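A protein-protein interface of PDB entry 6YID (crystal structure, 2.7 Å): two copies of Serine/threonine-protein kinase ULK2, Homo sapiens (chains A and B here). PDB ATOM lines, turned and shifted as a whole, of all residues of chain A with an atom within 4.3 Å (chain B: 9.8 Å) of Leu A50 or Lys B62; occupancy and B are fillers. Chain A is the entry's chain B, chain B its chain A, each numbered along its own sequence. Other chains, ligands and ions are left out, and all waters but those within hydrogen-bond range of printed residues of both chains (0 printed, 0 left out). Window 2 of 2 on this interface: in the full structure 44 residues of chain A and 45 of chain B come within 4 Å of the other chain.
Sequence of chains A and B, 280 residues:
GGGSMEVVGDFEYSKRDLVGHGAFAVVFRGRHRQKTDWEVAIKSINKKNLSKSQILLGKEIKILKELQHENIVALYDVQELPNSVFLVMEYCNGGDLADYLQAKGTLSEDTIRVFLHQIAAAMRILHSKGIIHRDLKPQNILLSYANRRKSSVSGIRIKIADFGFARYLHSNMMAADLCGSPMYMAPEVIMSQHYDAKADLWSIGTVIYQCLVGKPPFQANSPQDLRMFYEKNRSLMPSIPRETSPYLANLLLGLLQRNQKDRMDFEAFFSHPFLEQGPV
NZ of Lys B62 is in hydrogen-bond range of O of Ser A53 (2.7 Å).
The side-chain amino group of Lys B62 sits at hydrogen-bond distance from the backbone carbonyl oxygen of Ile A55 (3.3 Å).
The side-chain amino group (NZ) of Lys B62 is in hydrogen-bond range of the backbone carbonyl oxygen (O) of Leu A50, at 3.0 Å.
The backbone carbonyl oxygen (O) of Leu A50 lies within hydrogen-bond range of the side-chain hydroxyl (OG) of Ser A53 (2.7 Å).
The side-chain hydroxyl (OG) of Ser A53 is in hydrogen-bond range of the backbone NH (N) of Ile A55, 3.0 Å away.
The side-chain carboxylate of Glu B66 sits at hydrogen-bond distance from the side-chain hydroxyl of Tyr B168.
The backbone carbonyl oxygen (O) of Ala B166 lies within hydrogen-bond range of the side-chain amino group (NZ) of Lys B59, at 2.7 Å.
CD1 of Tyr B168 touches NE2 of Gln A54 (3.4 Å).
His B170 touches Gln A54.
CD2 of Leu A56 touches CG of Lys B59, 3.9 Å away.
Leu A56 touches Lys B62 (CD2 to CD, 3.9 Å).
Of the printed residues of chain B, Leu A50 touches Lys B62 (3.0 Å).
Of chain A, only Leu A50, Ser A53, Ile A55 and Leu A56 come within 4 Å of Lys B62.
No residue of chain B comes within 4 Å of Asn A49.
No residue of chain B comes within 4 Å of Ser A51.
Printed residues of chain B within 4 Å of Gln A54: Tyr B168 (3.4 Å) and His B170 (3.9 Å).
Printed residues of chain B within 4 Å of Ile A55: Lys B62 (3.3 Å).
Of the printed residues of chain A, Lys B59 touches Leu A56 (3.9 Å).
Printed residues of chain B within 4 Å of Leu A56: Lys B59 (3.9 Å) and Lys B62 (3.9 Å).
Printed residues of chain A within 4 Å of His B170: Gln A54.
Ile A45 touches none of the printed residues of chain B.
The nearest residue of chain B that does not touch Leu A50 is Glu B66 (7.2 Å).
Of the 13 printed residues of chain A, 5 touch a printed residue of chain B.
Hydrophobic or aromatic side chains of chain A within 4 Å of the printed part of chain B: Leu A56.
Printed residues of chain B that touch a printed residue of chain A: Lys B59, Lys B62, Tyr B168 and His B170.
Along chain B the printed residues that touch a printed residue of chain A span positions 59 to 170.
Among the printed residues, no Asp or Glu carboxylate lies within 4 Å of a Lys or Arg side-chain nitrogen of the other chain.
Positions printed for both chains: 56 and 57.
Of the 7 pairs that touch across the chains among the printed residues, none has its exchanged pair printed and touching as well.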
ATOM      1  N   ILE A  45      17.782  29.459  14.681  1.00  0.00           N
ATOM      2  CA  ILE A  45      16.649  28.544  14.584  1.00  0.00           C
ATOM      3  C   ILE A  45      16.300  28.058  15.990  1.00  0.00           C
ATOM      4  O   ILE A  45      17.093  27.370  16.632  1.00  0.00           O
ATOM      5  CB  ILE A  45      16.994  27.376  13.654  1.00  0.00           C
ATOM      6  CG1 ILE A  45      17.363  27.874  12.253  1.00  0.00           C
ATOM      7  CG2 ILE A  45      15.872  26.349  13.626  1.00  0.00           C
ATOM      8  CD1 ILE A  45      17.964  26.830  11.354  1.00  0.00           C
ATOM      9  N   ASN A  46      15.108  28.429  16.460  1.00  0.00           N
ATOM     10  CA  ASN A  46      14.645  28.017  17.786  1.00  0.00           C
ATOM     11  C   ASN A  46      14.417  26.503  17.775  1.00  0.00           C
ATOM     12  O   ASN A  46      13.713  26.004  16.927  1.00  0.00           O
ATOM     13  CB  ASN A  46      13.369  28.777  18.184  1.00  0.00           C
ATOM     14  CG  ASN A  46      12.825  28.328  19.520  1.00  0.00           C
ATOM     15  OD1 ASN A  46      11.903  27.529  19.574  1.00  0.00           O
ATOM     16  ND2 ASN A  46      13.437  28.780  20.603  1.00  0.00           N
ATOM     17  N   LYS A  47      14.998  25.792  18.745  1.00  0.00           N
ATOM     18  CA  LYS A  47      14.981  24.305  18.771  1.00  0.00           C
ATOM     19  C   LYS A  47      13.599  23.787  19.167  1.00  0.00           C
ATOM     20  O   LYS A  47      13.205  22.751  18.673  1.00  0.00           O
ATOM     21  CB  LYS A  47      16.057  23.737  19.701  1.00  0.00           C
ATOM     22  CG  LYS A  47      17.455  23.705  19.100  1.00  0.00           C
ATOM     23  CD  LYS A  47      18.549  23.415  20.100  1.00  0.00           C
ATOM     24  CE  LYS A  47      18.998  21.967  20.112  1.00  0.00           C
ATOM     25  NZ  LYS A  47      20.161  21.764  21.012  1.00  0.00           N
ATOM     26  N   LYS A  48      12.872  24.506  20.030  1.00  0.00           N
ATOM     27  CA  LYS A  48      11.535  24.043  20.486  1.00  0.00           C
ATOM     28  C   LYS A  48      10.508  24.211  19.364  1.00  0.00           C
ATOM     29  O   LYS A  48       9.685  23.331  19.152  1.00  0.00           O
ATOM     30  CB  LYS A  48      11.077  24.748  21.767  1.00  0.00           C
ATOM     31  CG  LYS A  48      11.473  24.013  23.034  1.00  0.00           C
ATOM     32  CD  LYS A  48      10.640  24.354  24.250  1.00  0.00           C
ATOM     33  CE  LYS A  48      11.229  23.778  25.524  1.00  0.00           C
ATOM     34  NZ  LYS A  48      11.043  24.683  26.690  1.00  0.00           N
ATOM     35  N   ASN A  49      10.576  25.327  18.636  1.00  0.00           N
ATOM     36  CA  ASN A  49       9.680  25.552  17.515  1.00  0.00           C
ATOM     37  C   ASN A  49       9.918  24.460  16.471  1.00  0.00           C
ATOM     38  O   ASN A  49       8.966  23.897  15.912  1.00  0.00           O
ATOM     39  CB  ASN A  49       9.852  26.937  16.890  1.00  0.00           C
ATOM     40  CG  ASN A  49       9.307  28.041  17.776  1.00  0.00           C
ATOM     41  OD1 ASN A  49       8.471  27.799  18.658  1.00  0.00           O
ATOM     42  ND2 ASN A  49       9.820  29.251  17.594  1.00  0.00           N
ATOM     43  N   LEU A  50      11.201  24.174  16.228  1.00  0.00           N
ATOM     44  CA  LEU A  50      11.619  23.255  15.204  1.00  0.00           C
ATOM     45  C   LEU A  50      11.147  21.833  15.533  1.00  0.00           C
ATOM     46  O   LEU A  50      10.827  21.066  14.620  1.00  0.00           O
ATOM     47  CB  LEU A  50      13.139  23.301  15.086  1.00  0.00           C
ATOM     48  CG  LEU A  50      13.736  22.394  14.016  1.00  0.00           C
ATOM     49  CD1 LEU A  50      13.253  22.825  12.637  1.00  0.00           C
ATOM     50  CD2 LEU A  50      15.257  22.413  14.102  1.00  0.00           C
ATOM     51  N   SER A  51      11.117  21.496  16.826  1.00  0.00           N
ATOM     52  CA  SER A  51      10.750  20.163  17.274  1.00  0.00           C
ATOM     53  C   SER A  51       9.236  19.956  17.183  1.00  0.00           C
ATOM     54  O   SER A  51       8.800  18.850  17.316  1.00  0.00           O
ATOM     55  CB  SER A  51      11.240  19.880  18.672  1.00  0.00           C
ATOM     56  OG  SER A  51      10.268  20.266  19.627  1.00  0.00           O
ATOM     57  N   LYS A  52       8.470  21.026  16.939  1.00  0.00           N
ATOM     58  CA  LYS A  52       7.004  20.940  16.717  1.00  0.00           C
ATOM     59  C   LYS A  52       6.678  20.926  15.220  1.00  0.00           C
ATOM     60  O   LYS A  52       5.527  20.877  14.869  1.00  0.00           O
ATOM     61  CB  LYS A  52       6.276  22.128  17.345  1.00  0.00           C
ATOM     62  CG  LYS A  52       6.317  22.241  18.855  1.00  0.00           C
ATOM     63  CD  LYS A  52       5.637  23.546  19.329  1.00  0.00           C
ATOM     64  CE  LYS A  52       5.772  23.813  20.815  1.00  0.00           C
ATOM     65  NZ  LYS A  52       4.522  24.374  21.399  1.00  0.00           N
ATOM     66  N   SER A  53       7.708  20.966  14.366  1.00  0.00           N
ATOM     67  CA  SER A  53       7.546  21.044  12.916  1.00  0.00           C
ATOM     68  C   SER A  53       7.969  19.726  12.283  1.00  0.00           C
ATOM     69  O   SER A  53       8.532  18.855  12.941  1.00  0.00           O
ATOM     70  CB  SER A  53       8.367  22.169  12.348  1.00  0.00           C
ATOM     71  OG  SER A  53       9.739  21.787  12.219  1.00  0.00           O
ATOM     72  N   GLN A  54       7.777  19.634  10.971  1.00  0.00           N
ATOM     73  CA  GLN A  54       8.233  18.489  10.227  1.00  0.00           C
ATOM     74  C   GLN A  54       9.496  18.862   9.432  1.00  0.00           C
ATOM     75  O   GLN A  54       9.847  18.201   8.470  1.00  0.00           O
ATOM     76  CB  GLN A  54       7.087  17.994   9.357  1.00  0.00           C
ATOM     77  CG  GLN A  54       5.831  17.685  10.166  1.00  0.00           C
ATOM     78  CD  GLN A  54       4.666  17.288   9.290  1.00  0.00           C
ATOM     79  OE1 GLN A  54       4.498  17.824   8.196  1.00  0.00           O
ATOM     80  NE2 GLN A  54       3.868  16.327   9.753  1.00  0.00           N
ATOM     81  N   ILE A  55      10.193  19.919   9.862  1.00  0.00           N
ATOM     82  CA  ILE A  55      11.406  20.374   9.204  1.00  0.00           C
ATOM     83  C   ILE A  55      12.555  19.459   9.619  1.00  0.00           C
ATOM     84  O   ILE A  55      12.740  19.186  10.813  1.00  0.00           O
ATOM     85  CB  ILE A  55      11.709  21.858   9.509  1.00  0.00           C
ATOM     86  CG1 ILE A  55      10.570  22.773   9.055  1.00  0.00           C
ATOM     87  CG2 ILE A  55      13.035  22.281   8.891  1.00  0.00           C
ATOM     88  CD1 ILE A  55      10.218  22.622   7.579  1.00  0.00           C
ATOM     89  N   LEU A  56      13.334  19.029   8.617  1.00  0.00           N
ATOM     90  CA  LEU A  56      14.508  18.193   8.802  1.00  0.00           C
ATOM     91  C   LEU A  56      15.765  19.037   8.578  1.00  0.00           C
ATOM     92  O   LEU A  56      16.347  19.019   7.519  1.00  0.00           O
ATOM     93  CB  LEU A  56      14.436  17.012   7.828  1.00  0.00           C
ATOM     94  CG  LEU A  56      13.077  16.311   7.784  1.00  0.00           C
ATOM     95  CD1 LEU A  56      13.017  15.251   6.697  1.00  0.00           C
ATOM     96  CD2 LEU A  56      12.760  15.705   9.139  1.00  0.00           C
ATOM     97  N   LEU A  57      16.199  19.735   9.622  1.00  0.00           N
ATOM     98  CA  LEU A  57      17.373  20.597   9.544  1.00  0.00           C
ATOM     99  C   LEU A  57      18.635  19.762   9.305  1.00  0.00           C
ATOM    100  O   LEU A  57      19.537  20.180   8.588  1.00  0.00           O
ATOM    101  CB  LEU A  57      17.479  21.407  10.840  1.00  0.00           C
ATOM    102  CG  LEU A  57      18.634  22.403  10.878  1.00  0.00           C
ATOM    103  CD1 LEU A  57      18.447  23.496   9.855  1.00  0.00           C
ATOM    104  CD2 LEU A  57      18.768  22.998  12.251  1.00  0.00           C
ATOM    105  N   LEU B  56      19.453   9.759   6.437  1.00  0.00           N
ATOM    106  CA  LEU B  56      19.113  10.889   7.235  1.00  0.00           C
ATOM    107  C   LEU B  56      18.895  10.451   8.684  1.00  0.00           C
ATOM    108  O   LEU B  56      17.776  10.278   9.132  1.00  0.00           O
ATOM    109  CB  LEU B  56      17.850  11.522   6.652  1.00  0.00           C
ATOM    110  CG  LEU B  56      17.909  11.811   5.157  1.00  0.00           C
ATOM    111  CD1 LEU B  56      16.610  12.430   4.683  1.00  0.00           C
ATOM    112  CD2 LEU B  56      19.074  12.730   4.829  1.00  0.00           C
ATOM    113  N   LEU B  57      19.990  10.366   9.435  1.00  0.00           N
ATOM    114  CA  LEU B  57      19.954   9.950  10.812  1.00  0.00           C
ATOM    115  C   LEU B  57      19.213  10.999  11.650  1.00  0.00           C
ATOM    116  O   LEU B  57      18.503  10.659  12.600  1.00  0.00           O
ATOM    117  CB  LEU B  57      21.391   9.758  11.320  1.00  0.00           C
ATOM    118  CG  LEU B  57      21.495   9.250  12.757  1.00  0.00           C
ATOM    119  CD1 LEU B  57      20.945   7.838  12.847  1.00  0.00           C
ATOM    120  CD2 LEU B  57      22.925   9.331  13.279  1.00  0.00           C
ATOM    121  N   GLY B  58      19.430  12.275  11.319  1.00  0.00           N
ATOM    122  CA  GLY B  58      18.732  13.375  11.932  1.00  0.00           C
ATOM    123  C   GLY B  58      17.227  13.159  11.931  1.00  0.00           C
ATOM    124  O   GLY B  58      16.556  13.418  12.918  1.00  0.00           O
ATOM    125  N   LYS B  59      16.705  12.655  10.814  1.00  0.00           N
ATOM    126  CA  LYS B  59      15.290  12.381  10.675  1.00  0.00           C
ATOM    127  C   LYS B  59      14.862  11.218  11.581  1.00  0.00           C
ATOM    128  O   LYS B  59      13.827  11.321  12.260  1.00  0.00           O
ATOM    129  CB  LYS B  59      14.950  12.063   9.224  1.00  0.00           C
ATOM    130  CG  LYS B  59      13.464  11.854   8.969  1.00  0.00           C
ATOM    131  CD  LYS B  59      13.223  11.132   7.653  1.00  0.00           C
ATOM    132  CE  LYS B  59      13.677   9.683   7.673  1.00  0.00           C
ATOM    133  NZ  LYS B  59      13.487   9.035   6.358  1.00  0.00           N
ATOM    134  N   GLU B  60      15.626  10.113  11.559  1.00  0.00           N
ATOM    135  CA  GLU B  60      15.309   8.947  12.383  1.00  0.00           C
ATOM    136  C   GLU B  60      15.246   9.373  13.859  1.00  0.00           C
ATOM    137  O   GLU B  60      14.343   8.968  14.588  1.00  0.00           O
ATOM    138  CB  GLU B  60      16.339   7.829  12.179  1.00  0.00           C
ATOM    139  CG  GLU B  60      16.320   7.221  10.785  1.00  0.00           C
ATOM    140  CD  GLU B  60      17.556   6.410  10.427  1.00  0.00           C
ATOM    141  OE1 GLU B  60      18.066   6.547   9.281  1.00  0.00           O
ATOM    142  OE2 GLU B  60      18.046   5.695  11.312  1.00  0.00           O
ATOM    143  N   ILE B  61      16.207  10.210  14.273  1.00  0.00           N
ATOM    144  CA  ILE B  61      16.308  10.664  15.652  1.00  0.00           C
ATOM    145  C   ILE B  61      15.118  11.560  15.998  1.00  0.00           C
ATOM    146  O   ILE B  61      14.552  11.443  17.077  1.00  0.00           O
ATOM    147  CB  ILE B  61      17.638  11.383  15.923  1.00  0.00           C
ATOM    148  CG1 ILE B  61      18.835  10.430  15.785  1.00  0.00           C
ATOM    149  CG2 ILE B  61      17.594  12.031  17.305  1.00  0.00           C
ATOM    150  CD1 ILE B  61      20.171  11.108  15.810  1.00  0.00           C
ATOM    151  N   LYS B  62      14.771  12.465  15.090  1.00  0.00           N
ATOM    152  CA  LYS B  62      13.675  13.402  15.308  1.00  0.00           C
ATOM    153  C   LYS B  62      12.369  12.623  15.471  1.00  0.00           C
ATOM    154  O   LYS B  62      11.557  12.939  16.319  1.00  0.00           O
ATOM    155  CB  LYS B  62      13.597  14.402  14.157  1.00  0.00           C
ATOM    156  CG  LYS B  62      12.376  15.311  14.147  1.00  0.00           C
ATOM    157  CD  LYS B  62      12.388  16.254  12.946  1.00  0.00           C
ATOM    158  CE  LYS B  62      11.105  17.033  12.783  1.00  0.00           C
ATOM    159  NZ  LYS B  62      11.142  18.293  13.553  1.00  0.00           N
ATOM    160  N   ILE B  63      12.195  11.582  14.660  1.00  0.00           N
ATOM    161  CA  ILE B  63      10.967  10.802  14.668  1.00  0.00           C
ATOM    162  C   ILE B  63      10.905   9.920  15.931  1.00  0.00           C
ATOM    163  O   ILE B  63       9.864   9.799  16.551  1.00  0.00           O
ATOM    164  CB  ILE B  63      10.857   9.996  13.371  1.00  0.00           C
ATOM    165  CG1 ILE B  63      10.463  10.909  12.206  1.00  0.00           C
ATOM    166  CG2 ILE B  63       9.898   8.843  13.538  1.00  0.00           C
ATOM    167  CD1 ILE B  63      10.643  10.282  10.842  1.00  0.00           C
ATOM    168  N   LEU B  64      12.030   9.315  16.308  1.00  0.00           N
ATOM    169  CA  LEU B  64      12.078   8.465  17.497  1.00  0.00           C
ATOM    170  C   LEU B  64      11.802   9.297  18.767  1.00  0.00           C
ATOM    171  O   LEU B  64      11.149   8.825  19.673  1.00  0.00           O
ATOM    172  CB  LEU B  64      13.442   7.776  17.562  1.00  0.00           C
ATOM    173  CG  LEU B  64      13.616   6.577  16.632  1.00  0.00           C
ATOM    174  CD1 LEU B  64      15.055   6.105  16.616  1.00  0.00           C
ATOM    175  CD2 LEU B  64      12.672   5.427  16.993  1.00  0.00           C
ATOM    176  N   LYS B  65      12.314  10.529  18.825  1.00  0.00           N
ATOM    177  CA  LYS B  65      12.101  11.434  19.972  1.00  0.00           C
ATOM    178  C   LYS B  65      10.614  11.790  20.074  1.00  0.00           C
ATOM    179  O   LYS B  65      10.063  11.878  21.143  1.00  0.00           O
ATOM    180  CB  LYS B  65      12.917  12.719  19.820  1.00  0.00           C
ATOM    181  CG  LYS B  65      14.390  12.614  20.180  1.00  0.00           C
ATOM    182  CD  LYS B  65      15.132  13.938  20.139  1.00  0.00           C
ATOM    183  CE  LYS B  65      14.493  15.010  21.003  1.00  0.00           C
ATOM    184  NZ  LYS B  65      15.478  16.036  21.412  1.00  0.00           N
ATOM    185  N   GLU B  66       9.982  11.999  18.923  1.00  0.00           N
ATOM    186  CA  GLU B  66       8.603  12.434  18.843  1.00  0.00           C
ATOM    187  C   GLU B  66       7.693  11.298  19.335  1.00  0.00           C
ATOM    188  O   GLU B  66       6.655  11.535  19.881  1.00  0.00           O
ATOM    189  CB  GLU B  66       8.315  12.865  17.402  1.00  0.00           C
ATOM    190  CG  GLU B  66       7.005  13.586  17.216  1.00  0.00           C
ATOM    191  CD  GLU B  66       6.866  14.338  15.894  1.00  0.00           C
ATOM    192  OE1 GLU B  66       5.727  14.705  15.541  1.00  0.00           O
ATOM    193  OE2 GLU B  66       7.886  14.571  15.226  1.00  0.00           O
ATOM    194  N   LEU B  67       8.104  10.053  19.090  1.00  0.00           N
ATOM    195  CA  LEU B  67       7.343   8.883  19.489  1.00  0.00           C
ATOM    196  C   LEU B  67       7.779   8.447  20.893  1.00  0.00           C
ATOM    197  O   LEU B  67       8.947   8.470  21.217  1.00  0.00           O
ATOM    198  CB  LEU B  67       7.567   7.778  18.458  1.00  0.00           C
ATOM    199  CG  LEU B  67       7.186   8.163  17.028  1.00  0.00           C
ATOM    200  CD1 LEU B  67       7.719   7.173  16.008  1.00  0.00           C
ATOM    201  CD2 LEU B  67       5.680   8.327  16.874  1.00  0.00           C
ATOM    202  N   GLN B  68       6.804   8.128  21.739  1.00  0.00           N
ATOM    203  CA  GLN B  68       7.074   7.600  23.035  1.00  0.00           C
ATOM    204  C   GLN B  68       5.935   6.661  23.402  1.00  0.00           C
ATOM    205  O   GLN B  68       4.922   7.084  23.886  1.00  0.00           O
ATOM    206  CB  GLN B  68       7.261   8.697  24.068  1.00  0.00           C
ATOM    207  CG  GLN B  68       7.777   8.142  25.391  1.00  0.00           C
ATOM    208  CD  GLN B  68       8.023   9.163  26.469  1.00  0.00           C
ATOM    209  OE1 GLN B  68       7.584   8.979  27.604  1.00  0.00           O
ATOM    210  NE2 GLN B  68       8.757  10.224  26.135  1.00  0.00           N
ATOM    211  N   LEU B  75      14.183   5.391  22.034  1.00  0.00           N
ATOM    212  CA  LEU B  75      15.494   6.016  21.995  1.00  0.00           C
ATOM    213  C   LEU B  75      15.693   6.755  23.324  1.00  0.00           C
ATOM    214  O   LEU B  75      14.912   7.652  23.650  1.00  0.00           O
ATOM    215  CB  LEU B  75      15.562   6.997  20.823  1.00  0.00           C
ATOM    216  CG  LEU B  75      16.856   7.787  20.694  1.00  0.00           C
ATOM    217  CD1 LEU B  75      18.007   6.867  20.438  1.00  0.00           C
ATOM    218  CD2 LEU B  75      16.763   8.828  19.589  1.00  0.00           C
ATOM    219  N   VAL B  78      21.455  10.045  22.655  1.00  0.00           N
ATOM    220  CA  VAL B  78      22.325  10.208  21.502  1.00  0.00           C
ATOM    221  C   VAL B  78      23.640  10.820  21.995  1.00  0.00           C
ATOM    222  O   VAL B  78      23.616  11.843  22.649  1.00  0.00           O
ATOM    223  CB  VAL B  78      21.663  11.090  20.437  1.00  0.00           C
ATOM    224  CG1 VAL B  78      22.500  11.172  19.179  1.00  0.00           C
ATOM    225  CG2 VAL B  78      20.263  10.595  20.110  1.00  0.00           C
ATOM    226  N   LEU B  87      23.602   5.666  19.325  1.00  0.00           N
ATOM    227  CA  LEU B  87      22.204   5.654  19.722  1.00  0.00           C
ATOM    228  C   LEU B  87      22.018   4.613  20.831  1.00  0.00           C
ATOM    229  O   LEU B  87      22.381   3.437  20.659  1.00  0.00           O
ATOM    230  CB  LEU B  87      21.360   5.312  18.496  1.00  0.00           C
ATOM    231  CG  LEU B  87      20.879   6.500  17.675  1.00  0.00           C
ATOM    232  CD1 LEU B  87      21.958   7.540  17.502  1.00  0.00           C
ATOM    233  CD2 LEU B  87      20.354   6.039  16.327  1.00  0.00           C
ATOM    234  N   LYS B 129       0.536  11.659  14.628  1.00  0.00           N
ATOM    235  CA  LYS B 129       1.684  12.568  14.394  1.00  0.00           C
ATOM    236  C   LYS B 129       1.934  12.773  12.894  1.00  0.00           C
ATOM    237  O   LYS B 129       2.858  13.469  12.526  1.00  0.00           O
ATOM    238  CB  LYS B 129       2.978  11.999  14.983  1.00  0.00           C
ATOM    239  CG  LYS B 129       2.923  11.545  16.434  1.00  0.00           C
ATOM    240  CD  LYS B 129       3.011  12.662  17.424  1.00  0.00           C
ATOM    241  CE  LYS B 129       3.144  12.153  18.834  1.00  0.00           C
ATOM    242  NZ  LYS B 129       3.216  13.288  19.776  1.00  0.00           N
ATOM    243  N   ILE B 131       3.050  10.508  10.630  1.00  0.00           N
ATOM    244  CA  ILE B 131       4.270   9.834  10.227  1.00  0.00           C
ATOM    245  C   ILE B 131       3.913   8.519   9.533  1.00  0.00           C
ATOM    246  O   ILE B 131       3.123   7.735  10.035  1.00  0.00           O
ATOM    247  CB  ILE B 131       5.177   9.569  11.436  1.00  0.00           C
ATOM    248  CG1 ILE B 131       5.634  10.873  12.085  1.00  0.00           C
ATOM    249  CG2 ILE B 131       6.361   8.682  11.034  1.00  0.00           C
ATOM    250  CD1 ILE B 131       6.322  10.700  13.414  1.00  0.00           C
ATOM    251  N   PHE B 163      13.048   3.670  11.307  1.00  0.00           N
ATOM    252  CA  PHE B 163      12.334   4.753  10.685  1.00  0.00           C
ATOM    253  C   PHE B 163      13.206   5.399   9.607  1.00  0.00           C
ATOM    254  O   PHE B 163      12.986   6.561   9.256  1.00  0.00           O
ATOM    255  CB  PHE B 163      11.856   5.718  11.769  1.00  0.00           C
ATOM    256  CG  PHE B 163      10.750   5.146  12.618  1.00  0.00           C
ATOM    257  CD1 PHE B 163      11.022   4.289  13.658  1.00  0.00           C
ATOM    258  CD2 PHE B 163       9.430   5.415  12.329  1.00  0.00           C
ATOM    259  CE1 PHE B 163       9.997   3.748  14.414  1.00  0.00           C
ATOM    260  CE2 PHE B 163       8.407   4.915  13.117  1.00  0.00           C
ATOM    261  CZ  PHE B 163       8.692   4.076  14.151  1.00  0.00           C
ATOM    262  N   ALA B 166      11.098   6.542   6.728  1.00  0.00           N
ATOM    263  CA  ALA B 166       9.858   7.174   7.196  1.00  0.00           C
ATOM    264  C   ALA B 166       9.765   8.601   6.660  1.00  0.00           C
ATOM    265  O   ALA B 166      10.773   9.203   6.275  1.00  0.00           O
ATOM    266  CB  ALA B 166       9.822   7.145   8.698  1.00  0.00           C
ATOM    267  N   ARG B 167       8.547   9.146   6.623  1.00  0.00           N
ATOM    268  CA  ARG B 167       8.365  10.512   6.215  1.00  0.00           C
ATOM    269  C   ARG B 167       7.107  11.088   6.870  1.00  0.00           C
ATOM    270  O   ARG B 167       6.278  10.358   7.391  1.00  0.00           O
ATOM    271  CB  ARG B 167       8.376  10.596   4.688  1.00  0.00           C
ATOM    272  CG  ARG B 167       7.022  10.670   3.999  1.00  0.00           C
ATOM    273  CD  ARG B 167       7.209  10.925   2.494  1.00  0.00           C
ATOM    274  NE  ARG B 167       5.929  11.006   1.792  1.00  0.00           N
ATOM    275  CZ  ARG B 167       5.105  12.047   1.849  1.00  0.00           C
ATOM    276  NH1 ARG B 167       5.552  13.224   2.226  1.00  0.00           N
ATOM    277  NH2 ARG B 167       3.813  11.886   1.641  1.00  0.00           N
ATOM    278  N   TYR B 168       7.070  12.424   6.943  1.00  0.00           N
ATOM    279  CA  TYR B 168       5.959  13.171   7.466  1.00  0.00           C
ATOM    280  C   TYR B 168       5.003  13.524   6.320  1.00  0.00           C
ATOM    281  O   TYR B 168       5.468  13.973   5.274  1.00  0.00           O
ATOM    282  CB  TYR B 168       6.433  14.472   8.116  1.00  0.00           C
ATOM    283  CG  TYR B 168       7.138  14.331   9.433  1.00  0.00           C
ATOM    284  CD1 TYR B 168       6.424  14.221  10.609  1.00  0.00           C
ATOM    285  CD2 TYR B 168       8.520  14.377   9.515  1.00  0.00           C
ATOM    286  CE1 TYR B 168       7.063  14.113  11.833  1.00  0.00           C
ATOM    287  CE2 TYR B 168       9.176  14.250  10.731  1.00  0.00           C
ATOM    288  CZ  TYR B 168       8.441  14.114  11.892  1.00  0.00           C
ATOM    289  OH  TYR B 168       9.069  14.008  13.098  1.00  0.00           O
ATOM    290  N   HIS B 170       2.631  16.041   4.603  1.00  0.00           N
ATOM    291  CA  HIS B 170       2.584  17.486   4.489  1.00  0.00           C
ATOM    292  C   HIS B 170       1.110  17.908   4.449  1.00  0.00           C
ATOM    293  O   HIS B 170       0.579  18.174   3.394  1.00  0.00           O
ATOM    294  CB  HIS B 170       3.449  17.933   3.291  1.00  0.00           C
ATOM    295  CG  HIS B 170       4.879  17.501   3.400  1.00  0.00           C
ATOM    296  ND1 HIS B 170       5.659  17.783   4.521  1.00  0.00           N
ATOM    297  CD2 HIS B 170       5.676  16.802   2.559  1.00  0.00           C
ATOM    298  CE1 HIS B 170       6.866  17.281   4.359  1.00  0.00           C
ATOM    299  NE2 HIS B 170       6.902  16.671   3.166  1.00  0.00           N
